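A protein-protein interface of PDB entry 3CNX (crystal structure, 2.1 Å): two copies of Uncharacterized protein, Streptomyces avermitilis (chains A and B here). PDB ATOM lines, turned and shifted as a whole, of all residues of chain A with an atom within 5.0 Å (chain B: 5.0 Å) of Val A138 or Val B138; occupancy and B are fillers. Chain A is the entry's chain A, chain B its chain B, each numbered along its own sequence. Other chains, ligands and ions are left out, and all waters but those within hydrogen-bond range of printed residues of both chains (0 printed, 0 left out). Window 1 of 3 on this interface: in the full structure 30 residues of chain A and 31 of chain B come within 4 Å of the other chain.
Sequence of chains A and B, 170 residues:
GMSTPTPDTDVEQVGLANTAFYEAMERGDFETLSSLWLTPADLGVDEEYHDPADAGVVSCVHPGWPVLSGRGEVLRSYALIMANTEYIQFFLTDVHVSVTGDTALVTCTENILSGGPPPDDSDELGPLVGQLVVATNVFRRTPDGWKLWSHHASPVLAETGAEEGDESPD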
ATOM      1  N   THR A 103      -3.966  32.212 -26.959  1.00  0.00           N
ATOM      2  CA  THR A 103      -5.221  32.084 -27.753  1.00  0.00           C
ATOM      3  C   THR A 103      -5.803  33.433 -28.113  1.00  0.00           C
ATOM      4  O   THR A 103      -5.801  34.356 -27.312  1.00  0.00           O
ATOM      5  CB  THR A 103      -6.291  31.294 -26.981  1.00  0.00           C
ATOM      6  OG1 THR A 103      -5.749  30.037 -26.579  1.00  0.00           O
ATOM      7  CG2 THR A 103      -7.508  31.030 -27.863  1.00  0.00           C
ATOM      8  N   ALA A 104      -6.293  33.547 -29.336  1.00  0.00           N
ATOM      9  CA  ALA A 104      -6.943  34.785 -29.767  1.00  0.00           C
ATOM     10  C   ALA A 104      -8.282  34.522 -30.409  1.00  0.00           C
ATOM     11  O   ALA A 104      -8.490  33.546 -31.112  1.00  0.00           O
ATOM     12  CB  ALA A 104      -6.019  35.615 -30.702  1.00  0.00           C
ATOM     13  N   LEU A 105      -9.199  35.415 -30.108  1.00  0.00           N
ATOM     14  CA  LEU A 105     -10.574  35.341 -30.553  1.00  0.00           C
ATOM     15  C   LEU A 105     -10.851  36.532 -31.433  1.00  0.00           C
ATOM     16  O   LEU A 105     -10.706  37.660 -30.989  1.00  0.00           O
ATOM     17  CB  LEU A 105     -11.489  35.398 -29.317  1.00  0.00           C
ATOM     18  CG  LEU A 105     -12.820  34.657 -29.258  1.00  0.00           C
ATOM     19  CD1 LEU A 105     -12.591  33.220 -29.551  1.00  0.00           C
ATOM     20  CD2 LEU A 105     -13.428  34.855 -27.844  1.00  0.00           C
ATOM     21  N   THR A 136     -16.901  33.868 -35.706  1.00  0.00           N
ATOM     22  CA  THR A 136     -15.949  33.765 -34.615  1.00  0.00           C
ATOM     23  C   THR A 136     -14.860  32.813 -35.019  1.00  0.00           C
ATOM     24  O   THR A 136     -15.087  31.633 -35.251  1.00  0.00           O
ATOM     25  CB  THR A 136     -16.584  33.208 -33.309  1.00  0.00           C
ATOM     26  OG1 THR A 136     -17.674  34.048 -32.928  1.00  0.00           O
ATOM     27  CG2 THR A 136     -15.553  33.176 -32.159  1.00  0.00           C
ATOM     28  N   ASN A 137     -13.659  33.369 -35.100  1.00  0.00           N
ATOM     29  CA  ASN A 137     -12.472  32.607 -35.412  1.00  0.00           C
ATOM     30  C   ASN A 137     -11.563  32.561 -34.181  1.00  0.00           C
ATOM     31  O   ASN A 137     -11.283  33.585 -33.539  1.00  0.00           O
ATOM     32  CB  ASN A 137     -11.745  33.259 -36.578  1.00  0.00           C
ATOM     33  CG  ASN A 137     -12.594  33.332 -37.846  1.00  0.00           C
ATOM     34  OD1 ASN A 137     -13.400  32.441 -38.145  1.00  0.00           O
ATOM     35  ND2 ASN A 137     -12.407  34.402 -38.608  1.00  0.00           N
ATOM     36  N   VAL A 138     -11.116  31.361 -33.866  1.00  0.00           N
ATOM     37  CA  VAL A 138     -10.228  31.135 -32.761  1.00  0.00           C
ATOM     38  C   VAL A 138      -8.861  30.731 -33.276  1.00  0.00           C
ATOM     39  O   VAL A 138      -8.721  29.756 -34.030  1.00  0.00           O
ATOM     40  CB  VAL A 138     -10.772  30.003 -31.821  1.00  0.00           C
ATOM     41  CG1 VAL A 138      -9.938  29.910 -30.538  1.00  0.00           C
ATOM     42  CG2 VAL A 138     -12.267  30.243 -31.490  1.00  0.00           C
ATOM     43  N   PHE A 139      -7.862  31.489 -32.831  1.00  0.00           N
ATOM     44  CA  PHE A 139      -6.471  31.283 -33.180  1.00  0.00           C
ATOM     45  C   PHE A 139      -5.629  30.861 -31.992  1.00  0.00           C
ATOM     46  O   PHE A 139      -5.853  31.207 -30.830  1.00  0.00           O
ATOM     47  CB  PHE A 139      -5.825  32.532 -33.787  1.00  0.00           C
ATOM     48  CG  PHE A 139      -6.424  32.944 -35.078  1.00  0.00           C
ATOM     49  CD1 PHE A 139      -7.540  33.774 -35.106  1.00  0.00           C
ATOM     50  CD2 PHE A 139      -5.893  32.503 -36.272  1.00  0.00           C
ATOM     51  CE1 PHE A 139      -8.109  34.159 -36.309  1.00  0.00           C
ATOM     52  CE2 PHE A 139      -6.462  32.878 -37.467  1.00  0.00           C
ATOM     53  CZ  PHE A 139      -7.568  33.706 -37.486  1.00  0.00           C
ATOM     54  N   ARG A 140      -4.624  30.106 -32.355  1.00  0.00           N
ATOM     55  CA  ARG A 140      -3.676  29.601 -31.398  1.00  0.00           C
ATOM     56  C   ARG A 140      -2.295  30.046 -31.817  1.00  0.00           C
ATOM     57  O   ARG A 140      -1.969  30.115 -33.007  1.00  0.00           O
ATOM     58  CB  ARG A 140      -3.776  28.094 -31.372  1.00  0.00           C
ATOM     59  CG  ARG A 140      -2.978  27.476 -30.278  1.00  0.00           C
ATOM     60  CD  ARG A 140      -3.777  27.531 -28.983  1.00  0.00           C
ATOM     61  NE  ARG A 140      -2.877  27.355 -27.844  1.00  0.00           N
ATOM     62  CZ  ARG A 140      -3.245  27.441 -26.576  1.00  0.00           C
ATOM     63  NH1 ARG A 140      -4.514  27.696 -26.269  1.00  0.00           N
ATOM     64  NH2 ARG A 140      -2.337  27.273 -25.623  1.00  0.00           N
ATOM     65  N   LYS A 147      -2.344  30.223 -35.718  1.00  0.00           N
ATOM     66  CA  LYS A 147      -3.032  29.214 -36.499  1.00  0.00           C
ATOM     67  C   LYS A 147      -4.496  29.082 -36.043  1.00  0.00           C
ATOM     68  O   LYS A 147      -4.794  29.220 -34.868  1.00  0.00           O
ATOM     69  CB  LYS A 147      -2.343  27.856 -36.313  1.00  0.00           C
ATOM     70  CG  LYS A 147      -0.859  27.838 -36.594  1.00  0.00           C
ATOM     71  CD  LYS A 147      -0.584  27.682 -38.070  1.00  0.00           C
ATOM     72  CE  LYS A 147       0.786  27.134 -38.300  1.00  0.00           C
ATOM     73  NZ  LYS A 147       1.196  27.513 -39.660  1.00  0.00           N
ATOM     74  N   LEU A 148      -5.366  28.801 -37.010  1.00  0.00           N
ATOM     75  CA  LEU A 148      -6.805  28.553 -36.783  1.00  0.00           C
ATOM     76  C   LEU A 148      -7.067  27.235 -36.072  1.00  0.00           C
ATOM     77  O   LEU A 148      -6.572  26.141 -36.418  1.00  0.00           O
ATOM     78  CB  LEU A 148      -7.636  28.590 -38.078  1.00  0.00           C
ATOM     79  CG  LEU A 148      -8.303  29.873 -38.540  1.00  0.00           C
ATOM     80  CD1 LEU A 148      -8.894  29.604 -39.921  1.00  0.00           C
ATOM     81  CD2 LEU A 148      -9.362  30.307 -37.562  1.00  0.00           C
ATOM     82  N   TRP A 149      -7.859  27.381 -35.047  1.00  0.00           N
ATOM     83  CA  TRP A 149      -8.291  26.255 -34.247  1.00  0.00           C
ATOM     84  C   TRP A 149      -9.736  26.011 -34.590  1.00  0.00           C
ATOM     85  O   TRP A 149     -10.199  24.876 -34.701  1.00  0.00           O
ATOM     86  CB  TRP A 149      -8.091  26.577 -32.771  1.00  0.00           C
ATOM     87  CG  TRP A 149      -8.380  25.500 -31.810  1.00  0.00           C
ATOM     88  CD1 TRP A 149      -8.720  24.225 -32.081  1.00  0.00           C
ATOM     89  CD2 TRP A 149      -8.307  25.613 -30.388  1.00  0.00           C
ATOM     90  NE1 TRP A 149      -8.894  23.525 -30.912  1.00  0.00           N
ATOM     91  CE2 TRP A 149      -8.617  24.354 -29.854  1.00  0.00           C
ATOM     92  CE3 TRP A 149      -7.979  26.660 -29.512  1.00  0.00           C
ATOM     93  CZ2 TRP A 149      -8.644  24.105 -28.474  1.00  0.00           C
ATOM     94  CZ3 TRP A 149      -8.015  26.421 -28.146  1.00  0.00           C
ATOM     95  CH2 TRP A 149      -8.360  25.155 -27.638  1.00  0.00           C
ATOM     96  N   SER A 150     -10.450  27.094 -34.775  1.00  0.00           N
ATOM     97  CA  SER A 150     -11.902  27.005 -35.029  1.00  0.00           C
ATOM     98  C   SER A 150     -12.368  28.164 -35.844  1.00  0.00           C
ATOM     99  O   SER A 150     -11.961  29.248 -35.581  1.00  0.00           O
ATOM    100  CB  SER A 150     -12.679  27.020 -33.710  1.00  0.00           C
ATOM    101  OG  SER A 150     -14.087  27.225 -33.916  1.00  0.00           O
ATOM    102  N   THR B 103      -7.122  27.168 -22.533  1.00  0.00           N
ATOM    103  CA  THR B 103      -8.319  27.304 -23.340  1.00  0.00           C
ATOM    104  C   THR B 103      -8.909  25.962 -23.718  1.00  0.00           C
ATOM    105  O   THR B 103      -8.221  24.996 -24.031  1.00  0.00           O
ATOM    106  CB  THR B 103      -8.103  28.102 -24.630  1.00  0.00           C
ATOM    107  OG1 THR B 103      -7.279  29.237 -24.390  1.00  0.00           O
ATOM    108  CG2 THR B 103      -9.410  28.588 -25.140  1.00  0.00           C
ATOM    109  N   ALA B 104     -10.227  25.940 -23.701  1.00  0.00           N
ATOM    110  CA  ALA B 104     -10.976  24.760 -24.112  1.00  0.00           C
ATOM    111  C   ALA B 104     -11.995  25.132 -25.167  1.00  0.00           C
ATOM    112  O   ALA B 104     -12.667  26.175 -25.104  1.00  0.00           O
ATOM    113  CB  ALA B 104     -11.656  24.068 -22.897  1.00  0.00           C
ATOM    114  N   LEU B 105     -12.084  24.260 -26.156  1.00  0.00           N
ATOM    115  CA  LEU B 105     -13.051  24.413 -27.235  1.00  0.00           C
ATOM    116  C   LEU B 105     -14.003  23.247 -27.205  1.00  0.00           C
ATOM    117  O   LEU B 105     -13.609  22.084 -27.253  1.00  0.00           O
ATOM    118  CB  LEU B 105     -12.339  24.431 -28.566  1.00  0.00           C
ATOM    119  CG  LEU B 105     -12.989  25.102 -29.756  1.00  0.00           C
ATOM    120  CD1 LEU B 105     -12.752  26.558 -29.634  1.00  0.00           C
ATOM    121  CD2 LEU B 105     -12.303  24.531 -31.004  1.00  0.00           C
ATOM    122  N   THR B 136     -20.273  26.387 -30.935  1.00  0.00           N
ATOM    123  CA  THR B 136     -18.900  26.402 -30.497  1.00  0.00           C
ATOM    124  C   THR B 136     -18.738  27.306 -29.264  1.00  0.00           C
ATOM    125  O   THR B 136     -18.909  28.522 -29.325  1.00  0.00           O
ATOM    126  CB  THR B 136     -17.976  26.876 -31.599  1.00  0.00           C
ATOM    127  OG1 THR B 136     -18.172  26.042 -32.745  1.00  0.00           O
ATOM    128  CG2 THR B 136     -16.516  26.763 -31.155  1.00  0.00           C
ATOM    129  N   ASN B 137     -18.380  26.673 -28.156  1.00  0.00           N
ATOM    130  CA  ASN B 137     -18.150  27.370 -26.884  1.00  0.00           C
ATOM    131  C   ASN B 137     -16.680  27.316 -26.521  1.00  0.00           C
ATOM    132  O   ASN B 137     -16.067  26.240 -26.495  1.00  0.00           O
ATOM    133  CB  ASN B 137     -18.951  26.731 -25.752  1.00  0.00           C
ATOM    134  CG  ASN B 137     -20.439  26.713 -26.006  1.00  0.00           C
ATOM    135  OD1 ASN B 137     -20.969  27.591 -26.683  1.00  0.00           O
ATOM    136  ND2 ASN B 137     -21.134  25.717 -25.436  1.00  0.00           N
ATOM    137  N   VAL B 138     -16.139  28.490 -26.213  1.00  0.00           N
ATOM    138  CA  VAL B 138     -14.730  28.649 -25.873  1.00  0.00           C
ATOM    139  C   VAL B 138     -14.647  29.034 -24.415  1.00  0.00           C
ATOM    140  O   VAL B 138     -15.164  30.075 -24.009  1.00  0.00           O
ATOM    141  CB  VAL B 138     -14.055  29.769 -26.724  1.00  0.00           C
ATOM    142  CG1 VAL B 138     -12.595  29.958 -26.304  1.00  0.00           C
ATOM    143  CG2 VAL B 138     -14.200  29.494 -28.236  1.00  0.00           C
ATOM    144  N   PHE B 139     -14.015  28.163 -23.641  1.00  0.00           N
ATOM    145  CA  PHE B 139     -13.794  28.349 -22.220  1.00  0.00           C
ATOM    146  C   PHE B 139     -12.349  28.673 -21.925  1.00  0.00           C
ATOM    147  O   PHE B 139     -11.397  28.343 -22.664  1.00  0.00           O
ATOM    148  CB  PHE B 139     -14.165  27.109 -21.375  1.00  0.00           C
ATOM    149  CG  PHE B 139     -15.593  26.697 -21.483  1.00  0.00           C
ATOM    150  CD1 PHE B 139     -16.019  25.919 -22.524  1.00  0.00           C
ATOM    151  CD2 PHE B 139     -16.505  27.075 -20.523  1.00  0.00           C
ATOM    152  CE1 PHE B 139     -17.328  25.549 -22.627  1.00  0.00           C
ATOM    153  CE2 PHE B 139     -17.817  26.688 -20.608  1.00  0.00           C
ATOM    154  CZ  PHE B 139     -18.229  25.939 -21.676  1.00  0.00           C
ATOM    155  N   ARG B 140     -12.227  29.278 -20.771  1.00  0.00           N
ATOM    156  CA  ARG B 140     -10.980  29.802 -20.274  1.00  0.00           C
ATOM    157  C   ARG B 140     -10.757  29.374 -18.813  1.00  0.00           C
ATOM    158  O   ARG B 140     -11.637  29.496 -17.949  1.00  0.00           O
ATOM    159  CB  ARG B 140     -11.058  31.314 -20.406  1.00  0.00           C
ATOM    160  CG  ARG B 140      -9.772  32.000 -20.271  1.00  0.00           C
ATOM    161  CD  ARG B 140      -8.842  31.673 -21.416  1.00  0.00           C
ATOM    162  NE  ARG B 140      -7.493  32.043 -20.998  1.00  0.00           N
ATOM    163  CZ  ARG B 140      -6.420  31.967 -21.759  1.00  0.00           C
ATOM    164  NH1 ARG B 140      -6.498  31.537 -23.009  1.00  0.00           N
ATOM    165  NH2 ARG B 140      -5.267  32.335 -21.251  1.00  0.00           N
ATOM    166  N   LYS B 147     -14.529  29.311 -17.424  1.00  0.00           N
ATOM    167  CA  LYS B 147     -15.440  30.410 -17.694  1.00  0.00           C
ATOM    168  C   LYS B 147     -15.558  30.599 -19.178  1.00  0.00           C
ATOM    169  O   LYS B 147     -14.585  30.453 -19.899  1.00  0.00           O
ATOM    170  CB  LYS B 147     -14.902  31.705 -17.085  1.00  0.00           C
ATOM    171  CG  LYS B 147     -14.573  31.613 -15.610  1.00  0.00           C
ATOM    172  CD  LYS B 147     -15.798  31.347 -14.786  1.00  0.00           C
ATOM    173  CE  LYS B 147     -15.534  31.634 -13.312  1.00  0.00           C
ATOM    174  NZ  LYS B 147     -16.789  31.802 -12.561  1.00  0.00           N
ATOM    175  N   LEU B 148     -16.762  30.929 -19.605  1.00  0.00           N
ATOM    176  CA  LEU B 148     -17.062  31.155 -21.013  1.00  0.00           C
ATOM    177  C   LEU B 148     -16.422  32.424 -21.495  1.00  0.00           C
ATOM    178  O   LEU B 148     -16.491  33.451 -20.860  1.00  0.00           O
ATOM    179  CB  LEU B 148     -18.545  31.258 -21.278  1.00  0.00           C
ATOM    180  CG  LEU B 148     -19.377  30.092 -21.797  1.00  0.00           C
ATOM    181  CD1 LEU B 148     -20.784  30.597 -21.965  1.00  0.00           C
ATOM    182  CD2 LEU B 148     -18.837  29.495 -23.097  1.00  0.00           C
ATOM    183  N   TRP B 149     -15.787  32.311 -22.651  1.00  0.00           N
ATOM    184  CA  TRP B 149     -15.200  33.446 -23.359  1.00  0.00           C
ATOM    185  C   TRP B 149     -16.053  33.804 -24.603  1.00  0.00           C
ATOM    186  O   TRP B 149     -16.279  34.953 -24.921  1.00  0.00           O
ATOM    187  CB  TRP B 149     -13.772  33.073 -23.733  1.00  0.00           C
ATOM    188  CG  TRP B 149     -12.945  34.136 -24.336  1.00  0.00           C
ATOM    189  CD1 TRP B 149     -13.243  35.447 -24.430  1.00  0.00           C
ATOM    190  CD2 TRP B 149     -11.624  33.981 -24.886  1.00  0.00           C
ATOM    191  NE1 TRP B 149     -12.198  36.127 -25.019  1.00  0.00           N
ATOM    192  CE2 TRP B 149     -11.191  35.245 -25.295  1.00  0.00           C
ATOM    193  CE3 TRP B 149     -10.770  32.899 -25.049  1.00  0.00           C
ATOM    194  CZ2 TRP B 149      -9.945  35.457 -25.879  1.00  0.00           C
ATOM    195  CZ3 TRP B 149      -9.540  33.106 -25.622  1.00  0.00           C
ATOM    196  CH2 TRP B 149      -9.134  34.373 -26.034  1.00  0.00           C
ATOM    197  N   SER B 150     -16.505  32.780 -25.289  1.00  0.00           N
ATOM    198  CA  SER B 150     -17.368  32.911 -26.457  1.00  0.00           C
ATOM    199  C   SER B 150     -18.389  31.790 -26.495  1.00  0.00           C
ATOM    200  O   SER B 150     -18.074  30.676 -26.225  1.00  0.00           O
ATOM    201  CB  SER B 150     -16.535  32.816 -27.724  1.00  0.00           C
ATOM    202  OG  SER B 150     -17.355  32.758 -28.874  1.00  0.00           O
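The side-chain hydroxyl (OG1) of Thr A103 sits at hydrogen-bond distance from the side-chain hydroxyl (OG1) of Thr B103 (2.8 Å).
NH1 of Arg A140 lies within hydrogen-bond range of OG1 of Thr A103, 2.7 Å away.
The backbone carbonyl oxygen (O) of Val A138 sits at hydrogen-bond distance from the backbone NH (N) of Trp A149, at 2.7 Å.
The backbone carbonyl oxygen (O) of Ser A150 is in hydrogen-bond range of the backbone NH (N) of Val A138, 2.8 Å away.
The backbone NH of Arg A140 lies within hydrogen-bond range of the backbone carbonyl oxygen of Lys A147.
NH1 of Arg B140 is in hydrogen-bond range of OG1 of Thr B103 (2.8 Å).
The backbone NH (N) of Trp B149 is in hydrogen-bond range of the backbone carbonyl oxygen (O) of Val B138 (2.7 Å).
Arg B140 touches Thr A103.
Trp B149 touches Thr A103.
NE1 of Trp B149 touches CD2 of Leu A105 (3.3 Å).
OG of Ser B150 touches CG2 of Thr A136, at 3.8 Å.
Val A138 touches Val B138.
Arg A140 touches Thr B103 (NH1 to OG1, 3.7 Å).
Thr B103 touches Trp A149.
NE1 of Trp A149 touches CD2 of Leu B105, at 3.6 Å.
Ser A150 touches Leu B105 (CB to CD2, 3.7 Å).
Ser A150 touches Thr B136 (OG to CG2, 3.7 Å).
Val A138 touches just one residue of chain B: Val B138 (3.9 Å).
Val B138 touches one residue of chain A.
Of the printed residues of chain A, Arg B140 touches Thr A103 (3.9 Å).
Of the printed residues of chain A, Thr B103 touches Thr A103, Arg A140 and Trp A149.
Leu A148 touches none of the printed residues of chain B.
The nearest residue of chain B that does not touch Val A138 is Leu B105 (4.2 Å).
Of the 12 printed residues of chain A, 7 touch a printed residue of chain B.
Printed residues of chain A that touch a printed residue of chain B: Thr A103, Leu A105, Thr A136, Val A138, Arg A140, Trp A149 and Ser A150.
Hydrophobic or aromatic side chains of chain B within 4 Å of the printed part of chain A: Leu B105, Val B138 and Trp B149.
Thr B103 touches its own counterpart, Thr A103.
Thr A103 touches Arg B140, and with the chains exchanged Arg A140 touches Thr B103.
Thr A103 touches Trp B149, and with the chains exchanged Trp A149 touches Thr B103.
Leu A105 touches Ser B150, and with the chains exchanged Ser A150 touches Leu B105.
Positions printed for both chains: 103, 104, 105, 136, 137, 138, 139, 140, 147, 148, 149 and 150.
Of the 12 pairs that touch across the chains among the printed residues, 12 have their exchanged pair printed and touching as well.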
